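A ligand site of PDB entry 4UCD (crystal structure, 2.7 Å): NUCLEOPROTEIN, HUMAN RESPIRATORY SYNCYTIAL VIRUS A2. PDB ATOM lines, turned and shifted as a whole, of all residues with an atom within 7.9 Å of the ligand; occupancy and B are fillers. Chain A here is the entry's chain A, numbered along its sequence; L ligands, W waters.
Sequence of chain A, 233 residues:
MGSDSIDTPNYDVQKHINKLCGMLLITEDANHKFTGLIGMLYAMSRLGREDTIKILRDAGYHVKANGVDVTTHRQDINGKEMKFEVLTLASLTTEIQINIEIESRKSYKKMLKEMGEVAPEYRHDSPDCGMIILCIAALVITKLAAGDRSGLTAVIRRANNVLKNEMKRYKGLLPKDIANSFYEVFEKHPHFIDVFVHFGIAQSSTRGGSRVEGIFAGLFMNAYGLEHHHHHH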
ATOM      1  N   LYS A  19     -24.362  10.423   3.751  1.00  0.00           N
ATOM      2  CA  LYS A  19     -23.767   9.741   4.915  1.00  0.00           C
ATOM      3  C   LYS A  19     -24.072  10.540   6.200  1.00  0.00           C
ATOM      4  O   LYS A  19     -24.338   9.962   7.242  1.00  0.00           O
ATOM      5  CB  LYS A  19     -22.247   9.547   4.697  1.00  0.00           C
ATOM      6  CG  LYS A  19     -21.525   8.813   5.811  1.00  0.00           C
ATOM      7  CD  LYS A  19     -20.036   8.686   5.534  1.00  0.00           C
ATOM      8  CE  LYS A  19     -19.673   7.583   4.531  1.00  0.00           C
ATOM      9  NZ  LYS A  19     -20.086   7.878   3.112  1.00  0.00           N
ATOM     10  N   GLY A  22     -27.520   9.725   7.031  1.00  0.00           N
ATOM     11  CA  GLY A  22     -27.508   8.379   7.599  1.00  0.00           C
ATOM     12  C   GLY A  22     -27.043   8.303   9.037  1.00  0.00           C
ATOM     13  O   GLY A  22     -27.549   7.508   9.827  1.00  0.00           O
ATOM     14  N   MET A  23     -26.079   9.149   9.385  1.00  0.00           N
ATOM     15  CA  MET A  23     -25.539   9.264  10.731  1.00  0.00           C
ATOM     16  C   MET A  23     -26.603   9.709  11.693  1.00  0.00           C
ATOM     17  O   MET A  23     -26.718   9.137  12.772  1.00  0.00           O
ATOM     18  CB  MET A  23     -24.301  10.158  10.777  1.00  0.00           C
ATOM     19  CG  MET A  23     -23.084   9.500  10.135  1.00  0.00           C
ATOM     20  SD  MET A  23     -21.576  10.454  10.410  1.00  0.00           S
ATOM     21  CE  MET A  23     -21.562  11.548   9.060  1.00  0.00           C
ATOM     22  N   ILE A  26     -29.324   6.781  12.178  1.00  0.00           N
ATOM     23  CA  ILE A  26     -28.960   5.679  13.080  1.00  0.00           C
ATOM     24  C   ILE A  26     -28.798   6.166  14.540  1.00  0.00           C
ATOM     25  O   ILE A  26     -28.570   5.343  15.429  1.00  0.00           O
ATOM     26  CB  ILE A  26     -27.739   4.845  12.595  1.00  0.00           C
ATOM     27  CG1 ILE A  26     -26.396   5.594  12.752  1.00  0.00           C
ATOM     28  CG2 ILE A  26     -27.924   4.300  11.173  1.00  0.00           C
ATOM     29  CD1 ILE A  26     -25.195   4.672  13.026  1.00  0.00           C
ATOM     30  N   THR A  27     -28.902   7.489  14.803  1.00  0.00           N
ATOM     31  CA  THR A  27     -28.701   7.985  16.159  1.00  0.00           C
ATOM     32  C   THR A  27     -29.959   7.881  17.033  1.00  0.00           C
ATOM     33  O   THR A  27     -30.995   8.497  16.721  1.00  0.00           O
ATOM     34  CB  THR A  27     -28.091   9.417  16.195  1.00  0.00           C
ATOM     35  OG1 THR A  27     -26.898   9.429  15.413  1.00  0.00           O
ATOM     36  CG2 THR A  27     -27.752   9.872  17.595  1.00  0.00           C
ATOM     37  N   PHE A  84     -11.498  13.400  11.029  1.00  0.00           N
ATOM     38  CA  PHE A  84     -12.876  13.478  10.580  1.00  0.00           C
ATOM     39  C   PHE A  84     -12.971  14.105   9.211  1.00  0.00           C
ATOM     40  O   PHE A  84     -12.280  15.092   8.937  1.00  0.00           O
ATOM     41  CB  PHE A  84     -13.728  14.284  11.562  1.00  0.00           C
ATOM     42  CG  PHE A  84     -13.861  13.678  12.940  1.00  0.00           C
ATOM     43  CD1 PHE A  84     -12.950  13.975  13.935  1.00  0.00           C
ATOM     44  CD2 PHE A  84     -14.920  12.828  13.239  1.00  0.00           C
ATOM     45  CE1 PHE A  84     -13.077  13.403  15.199  1.00  0.00           C
ATOM     46  CE2 PHE A  84     -15.040  12.251  14.498  1.00  0.00           C
ATOM     47  CZ  PHE A  84     -14.115  12.534  15.468  1.00  0.00           C
ATOM     48  N   ILE A 100     -22.183  15.113  15.286  1.00  0.00           N
ATOM     49  CA  ILE A 100     -23.150  14.222  14.648  1.00  0.00           C
ATOM     50  C   ILE A 100     -22.432  12.856  14.422  1.00  0.00           C
ATOM     51  O   ILE A 100     -23.013  11.815  14.735  1.00  0.00           O
ATOM     52  CB  ILE A 100     -23.695  14.865  13.343  1.00  0.00           C
ATOM     53  CG1 ILE A 100     -24.685  16.023  13.668  1.00  0.00           C
ATOM     54  CG2 ILE A 100     -24.293  13.805  12.401  1.00  0.00           C
ATOM     55  CD1 ILE A 100     -25.239  16.834  12.459  1.00  0.00           C
ATOM     56  N   GLU A 101     -21.158  12.875  13.968  1.00  0.00           N
ATOM     57  CA  GLU A 101     -20.384  11.643  13.749  1.00  0.00           C
ATOM     58  C   GLU A 101     -20.109  10.907  15.073  1.00  0.00           C
ATOM     59  O   GLU A 101     -20.261   9.691  15.125  1.00  0.00           O
ATOM     60  CB  GLU A 101     -19.076  11.911  12.976  1.00  0.00           C
ATOM     61  CG  GLU A 101     -18.341  10.643  12.558  1.00  0.00           C
ATOM     62  CD  GLU A 101     -17.111  10.830  11.687  1.00  0.00           C
ATOM     63  OE1 GLU A 101     -17.090  11.760  10.833  1.00  0.00           O
ATOM     64  OE2 GLU A 101     -16.160  10.045  11.860  1.00  0.00           O
ATOM     65  N   ILE A 102     -19.721  11.629  16.120  1.00  0.00           N
ATOM     66  CA  ILE A 102     -19.459  11.050  17.454  1.00  0.00           C
ATOM     67  C   ILE A 102     -20.691  10.330  18.007  1.00  0.00           C
ATOM     68  O   ILE A 102     -20.589   9.163  18.385  1.00  0.00           O
ATOM     69  CB  ILE A 102     -18.908  12.112  18.444  1.00  0.00           C
ATOM     70  CG1 ILE A 102     -17.496  12.569  17.998  1.00  0.00           C
ATOM     71  CG2 ILE A 102     -18.904  11.593  19.878  1.00  0.00           C
ATOM     72  CD1 ILE A 102     -16.991  13.840  18.714  1.00  0.00           C
ATOM     73  N   GLU A 103     -21.842  11.019  18.051  1.00  0.00           N
ATOM     74  CA  GLU A 103     -23.113  10.474  18.547  1.00  0.00           C
ATOM     75  C   GLU A 103     -23.565   9.234  17.744  1.00  0.00           C
ATOM     76  O   GLU A 103     -24.008   8.264  18.347  1.00  0.00           O
ATOM     77  CB  GLU A 103     -24.197  11.576  18.588  1.00  0.00           C
ATOM     78  CG  GLU A 103     -23.972  12.650  19.635  1.00  0.00           C
ATOM     79  CD  GLU A 103     -23.733  12.191  21.072  1.00  0.00           C
ATOM     80  OE1 GLU A 103     -24.542  11.384  21.589  1.00  0.00           O
ATOM     81  OE2 GLU A 103     -22.748  12.655  21.687  1.00  0.00           O
ATOM     82  N   SER A 104     -23.421   9.260  16.397  1.00  0.00           N
ATOM     83  CA  SER A 104     -23.792   8.122  15.567  1.00  0.00           C
ATOM     84  C   SER A 104     -22.899   6.908  15.823  1.00  0.00           C
ATOM     85  O   SER A 104     -23.397   5.776  15.866  1.00  0.00           O
ATOM     86  CB  SER A 104     -23.881   8.473  14.083  1.00  0.00           C
ATOM     87  OG  SER A 104     -22.622   8.722  13.484  1.00  0.00           O
ATOM     88  N   ARG A 105     -21.588   7.150  16.074  1.00  0.00           N
ATOM     89  CA  ARG A 105     -20.611   6.113  16.371  1.00  0.00           C
ATOM     90  C   ARG A 105     -20.935   5.400  17.695  1.00  0.00           C
ATOM     91  O   ARG A 105     -20.753   4.187  17.797  1.00  0.00           O
ATOM     92  CB  ARG A 105     -19.192   6.679  16.329  1.00  0.00           C
ATOM     93  CG  ARG A 105     -18.631   6.803  14.902  1.00  0.00           C
ATOM     94  CD  ARG A 105     -17.162   7.206  14.936  1.00  0.00           C
ATOM     95  NE  ARG A 105     -16.511   7.285  13.625  1.00  0.00           N
ATOM     96  CZ  ARG A 105     -15.808   6.306  13.080  1.00  0.00           C
ATOM     97  NH1 ARG A 105     -15.656   5.151  13.710  1.00  0.00           N
ATOM     98  NH2 ARG A 105     -15.227   6.476  11.893  1.00  0.00           N
ATOM     99  N   LYS A 106     -21.482   6.154  18.683  1.00  0.00           N
ATOM    100  CA  LYS A 106     -21.950   5.640  19.982  1.00  0.00           C
ATOM    101  C   LYS A 106     -23.154   4.723  19.745  1.00  0.00           C
ATOM    102  O   LYS A 106     -23.192   3.641  20.311  1.00  0.00           O
ATOM    103  CB  LYS A 106     -22.379   6.781  20.925  1.00  0.00           C
ATOM    104  CG  LYS A 106     -21.266   7.553  21.593  1.00  0.00           C
ATOM    105  CD  LYS A 106     -21.844   8.555  22.599  1.00  0.00           C
ATOM    106  CE  LYS A 106     -20.913   9.695  22.922  1.00  0.00           C
ATOM    107  NZ  LYS A 106     -21.568  10.701  23.810  1.00  0.00           N
ATOM    108  N   SER A 107     -24.128   5.143  18.919  1.00  0.00           N
ATOM    109  CA  SER A 107     -25.303   4.352  18.571  1.00  0.00           C
ATOM    110  C   SER A 107     -24.917   3.065  17.811  1.00  0.00           C
ATOM    111  O   SER A 107     -25.492   1.994  18.067  1.00  0.00           O
ATOM    112  CB  SER A 107     -26.302   5.177  17.760  1.00  0.00           C
ATOM    113  OG  SER A 107     -27.070   6.008  18.606  1.00  0.00           O
ATOM    114  N   TYR A 108     -23.932   3.185  16.894  1.00  0.00           N
ATOM    115  CA  TYR A 108     -23.458   2.082  16.083  1.00  0.00           C
ATOM    116  C   TYR A 108     -22.825   0.989  16.946  1.00  0.00           C
ATOM    117  O   TYR A 108     -23.066  -0.192  16.678  1.00  0.00           O
ATOM    118  CB  TYR A 108     -22.467   2.592  15.017  1.00  0.00           C
ATOM    119  CG  TYR A 108     -22.004   1.516  14.079  1.00  0.00           C
ATOM    120  CD1 TYR A 108     -22.786   1.132  12.993  1.00  0.00           C
ATOM    121  CD2 TYR A 108     -20.793   0.851  14.268  1.00  0.00           C
ATOM    122  CE1 TYR A 108     -22.370   0.120  12.121  1.00  0.00           C
ATOM    123  CE2 TYR A 108     -20.362  -0.153  13.409  1.00  0.00           C
ATOM    124  CZ  TYR A 108     -21.162  -0.504  12.327  1.00  0.00           C
ATOM    125  OH  TYR A 108     -20.726  -1.468  11.456  1.00  0.00           O
ATOM    126  N   LYS A 109     -22.023   1.365  17.954  1.00  0.00           N
ATOM    127  CA  LYS A 109     -21.404   0.406  18.864  1.00  0.00           C
ATOM    128  C   LYS A 109     -22.457  -0.360  19.641  1.00  0.00           C
ATOM    129  O   LYS A 109     -22.327  -1.577  19.845  1.00  0.00           O
ATOM    130  CB  LYS A 109     -20.393   1.097  19.803  1.00  0.00           C
ATOM    131  CG  LYS A 109     -19.371   0.123  20.409  1.00  0.00           C
ATOM    132  CD  LYS A 109     -18.406   0.812  21.383  1.00  0.00           C
ATOM    133  CE  LYS A 109     -17.749  -0.161  22.351  1.00  0.00           C
ATOM    134  NZ  LYS A 109     -18.613  -0.449  23.528  1.00  0.00           N
ATOM    135  N   MET A 111     -25.503  -1.017  18.604  1.00  0.00           N
ATOM    136  CA  MET A 111     -26.086  -1.883  17.566  1.00  0.00           C
ATOM    137  C   MET A 111     -25.232  -3.135  17.410  1.00  0.00           C
ATOM    138  O   MET A 111     -25.808  -4.229  17.377  1.00  0.00           O
ATOM    139  CB  MET A 111     -26.179  -1.176  16.203  1.00  0.00           C
ATOM    140  CG  MET A 111     -27.183  -0.064  16.171  1.00  0.00           C
ATOM    141  SD  MET A 111     -27.217   0.857  14.568  1.00  0.00           S
ATOM    142  CE  MET A 111     -27.987  -0.406  13.463  1.00  0.00           C
ATOM    143  N   LEU A 112     -23.872  -2.990  17.316  1.00  0.00           N
ATOM    144  CA  LEU A 112     -22.978  -4.138  17.189  1.00  0.00           C
ATOM    145  C   LEU A 112     -23.155  -5.059  18.387  1.00  0.00           C
ATOM    146  O   LEU A 112     -23.273  -6.270  18.225  1.00  0.00           O
ATOM    147  CB  LEU A 112     -21.498  -3.732  17.089  1.00  0.00           C
ATOM    148  CG  LEU A 112     -21.008  -2.971  15.856  1.00  0.00           C
ATOM    149  CD1 LEU A 112     -19.590  -2.556  16.053  1.00  0.00           C
ATOM    150  CD2 LEU A 112     -21.110  -3.800  14.585  1.00  0.00           C
ATOM    151  N   GLU A 117     -22.482  -7.604  13.459  1.00  0.00           N
ATOM    152  CA  GLU A 117     -22.330  -6.705  12.304  1.00  0.00           C
ATOM    153  C   GLU A 117     -23.664  -6.342  11.681  1.00  0.00           C
ATOM    154  O   GLU A 117     -24.568  -7.170  11.627  1.00  0.00           O
ATOM    155  CB  GLU A 117     -21.329  -7.220  11.271  1.00  0.00           C
ATOM    156  CG  GLU A 117     -19.885  -6.873  11.594  1.00  0.00           C
ATOM    157  CD  GLU A 117     -19.479  -5.414  11.498  1.00  0.00           C
ATOM    158  OE1 GLU A 117     -20.286  -4.584  10.994  1.00  0.00           O
ATOM    159  OE2 GLU A 117     -18.351  -5.080  11.931  1.00  0.00           O
ATOM    160  N   VAL A 118     -23.792  -5.097  11.291  1.00  0.00           N
ATOM    161  CA  VAL A 118     -24.997  -4.491  10.780  1.00  0.00           C
ATOM    162  C   VAL A 118     -25.178  -4.660   9.235  1.00  0.00           C
ATOM    163  O   VAL A 118     -24.246  -4.425   8.479  1.00  0.00           O
ATOM    164  CB  VAL A 118     -24.991  -3.007  11.237  1.00  0.00           C
ATOM    165  CG1 VAL A 118     -26.235  -2.261  10.791  1.00  0.00           C
ATOM    166  CG2 VAL A 118     -24.798  -2.895  12.755  1.00  0.00           C
ATOM    167  N   ARG A 123     -27.369   0.557   8.028  1.00  0.00           N
ATOM    168  CA  ARG A 123     -26.201   1.415   8.236  1.00  0.00           C
ATOM    169  C   ARG A 123     -26.445   2.862   7.837  1.00  0.00           C
ATOM    170  O   ARG A 123     -27.341   3.154   7.055  1.00  0.00           O
ATOM    171  CB  ARG A 123     -25.008   0.853   7.444  1.00  0.00           C
ATOM    172  CG  ARG A 123     -24.404  -0.391   8.041  1.00  0.00           C
ATOM    173  CD  ARG A 123     -23.404  -0.988   7.078  1.00  0.00           C
ATOM    174  NE  ARG A 123     -22.355  -0.023   6.720  1.00  0.00           N
ATOM    175  CZ  ARG A 123     -21.252   0.192   7.426  1.00  0.00           C
ATOM    176  NH1 ARG A 123     -21.024  -0.476   8.541  1.00  0.00           N
ATOM    177  NH2 ARG A 123     -20.364   1.080   7.008  1.00  0.00           N
ATOM    178  N   HIS A 124     -25.560   3.754   8.337  1.00  0.00           N
ATOM    179  CA  HIS A 124     -25.506   5.207   8.065  1.00  0.00           C
ATOM    180  C   HIS A 124     -25.165   5.527   6.595  1.00  0.00           C
ATOM    181  O   HIS A 124     -25.399   6.647   6.148  1.00  0.00           O
ATOM    182  CB  HIS A 124     -24.452   5.885   8.996  1.00  0.00           C
ATOM    183  CG  HIS A 124     -23.049   5.477   8.711  1.00  0.00           C
ATOM    184  ND1 HIS A 124     -22.568   4.209   9.047  1.00  0.00           N
ATOM    185  CD2 HIS A 124     -22.064   6.168   8.078  1.00  0.00           C
ATOM    186  CE1 HIS A 124     -21.320   4.175   8.608  1.00  0.00           C
ATOM    187  NE2 HIS A 124     -20.967   5.334   8.038  1.00  0.00           N
ATOM    188  N   ASP A 125     -24.540   4.586   5.885  1.00  0.00           N
ATOM    189  CA  ASP A 125     -24.129   4.782   4.501  1.00  0.00           C
ATOM    190  C   ASP A 125     -25.025   4.078   3.462  1.00  0.00           C
ATOM    191  O   ASP A 125     -24.624   3.932   2.309  1.00  0.00           O
ATOM    192  CB  ASP A 125     -22.658   4.416   4.319  1.00  0.00           C
ATOM    193  CG  ASP A 125     -22.257   3.012   4.729  1.00  0.00           C
ATOM    194  OD1 ASP A 125     -23.167   2.180   4.980  1.00  0.00           O
ATOM    195  OD2 ASP A 125     -21.043   2.724   4.758  1.00  0.00           O
HETATM  196 CL1  LIG L   1     -21.397   5.686  12.564  1.00  0.00          CL
HETATM  197  C1  LIG L   1     -19.989   5.806  11.554  1.00  0.00           C
HETATM  198  C2  LIG L   1     -19.597   7.061  11.112  1.00  0.00           C
HETATM  199  C3  LIG L   1     -18.448   7.179  10.346  1.00  0.00           C
HETATM  200  C4  LIG L   1     -19.283   4.654  11.217  1.00  0.00           C
HETATM  201  C5  LIG L   1     -18.177   4.808  10.386  1.00  0.00           C
HETATM  202  C6  LIG L   1     -17.753   6.056   9.970  1.00  0.00           C
HETATM  203  C7  LIG L   1     -19.710   3.301  11.739  1.00  0.00           C
HETATM  204  N1  LIG L   1     -18.718   2.252  11.484  1.00  0.00           N
HETATM  205  N2  LIG L   1     -18.803   1.576  10.301  1.00  0.00           N
HETATM  206  C8  LIG L   1     -17.767   0.722  10.330  1.00  0.00           C
HETATM  207  C9  LIG L   1     -17.506  -0.281   9.223  1.00  0.00           C
HETATM  208  O1  LIG L   1     -17.871   0.066   8.072  1.00  0.00           O
HETATM  209  O2  LIG L   1     -16.966  -1.368   9.530  1.00  0.00           O
HETATM  210  C10 LIG L   1     -17.030   0.855  11.505  1.00  0.00           C
HETATM  211  C11 LIG L   1     -17.657   1.837  12.232  1.00  0.00           C
HETATM  212  C12 LIG L   1     -17.222   2.340  13.601  1.00  0.00           C
HETATM  213  O3  LIG L   1     -17.884   3.262  14.137  1.00  0.00           O
HETATM  214  O4  LIG L   1     -16.215   1.779  14.102  1.00  0.00           O
HETATM  215  O   HOH W   1     -17.940  -2.262  12.419  1.00  0.00           O
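NH2 of Arg 123 is in salt-bridge range of O1 of the ligand (2.9 Å).
The guanidinium group of Arg 105 is in salt-bridge range of an oxygen (O3) of the ligand, at 3.0 Å.
The side-chain hydroxyl (OH) of Tyr 108 lies within hydrogen-bond range of the guanidinium group (NH1) of Arg 123 (3.1 Å).
The side-chain carboxylate of Asp 125 lies within salt-bridge range of the guanidinium group of Arg 123, 2.9 Å away.
OE2 of Glu 101 lies within salt-bridge range of NE of Arg 105 (3.3 Å).
The side-chain hydroxyl of Ser 104 is in hydrogen-bond range of the backbone carbonyl oxygen of Glu 101, at 3.0 Å.
OG of Ser 104 lies close to SD of Met 23 (3.7 Å).
The side-chain hydroxyl (OG) of Ser 104 is in hydrogen-bond range of the backbone carbonyl oxygen (O) of Ile 100 (3.4 Å).
The side-chain hydroxyl (OH) of Tyr 108 sits at hydrogen-bond distance from the side-chain carboxylate (OE1) of Glu 117 (3.2 Å).
The side-chain hydroxyl (OG1) of Thr 27 lies within hydrogen-bond range of the backbone carbonyl oxygen (O) of Met 23 (2.7 Å).
Met 23 touches the ligand.
CD1 of Ile 26 touches CL1 of the ligand, at 3.96 Å.
Glu 101 touches the ligand (OE2 to C3, 3.97 Å).
Ser 104 touches the ligand (OG to CL1, 3.4 Å).
Tyr 108 touches the ligand.
His 124 touches the ligand (CE1 to C4, 3.3 Å).
Hydrophobic or aromatic side chains within 4 Å of the ligand: Met 23, Ile 26, Tyr 108 and His 124.
Of the 23 residues printed, 8 come within 4 Å of the ligand.
The nearest printed residue that does not touch the ligand is Glu 117 (4.6 Å).
Water W1 lies within hydrogen-bond range of the side-chain carboxylate of Glu 117 (2.9 Å), the side-chain hydroxyl of Tyr 108 (3.1 Å) and an oxygen (O2) of the ligand (3.2 Å).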
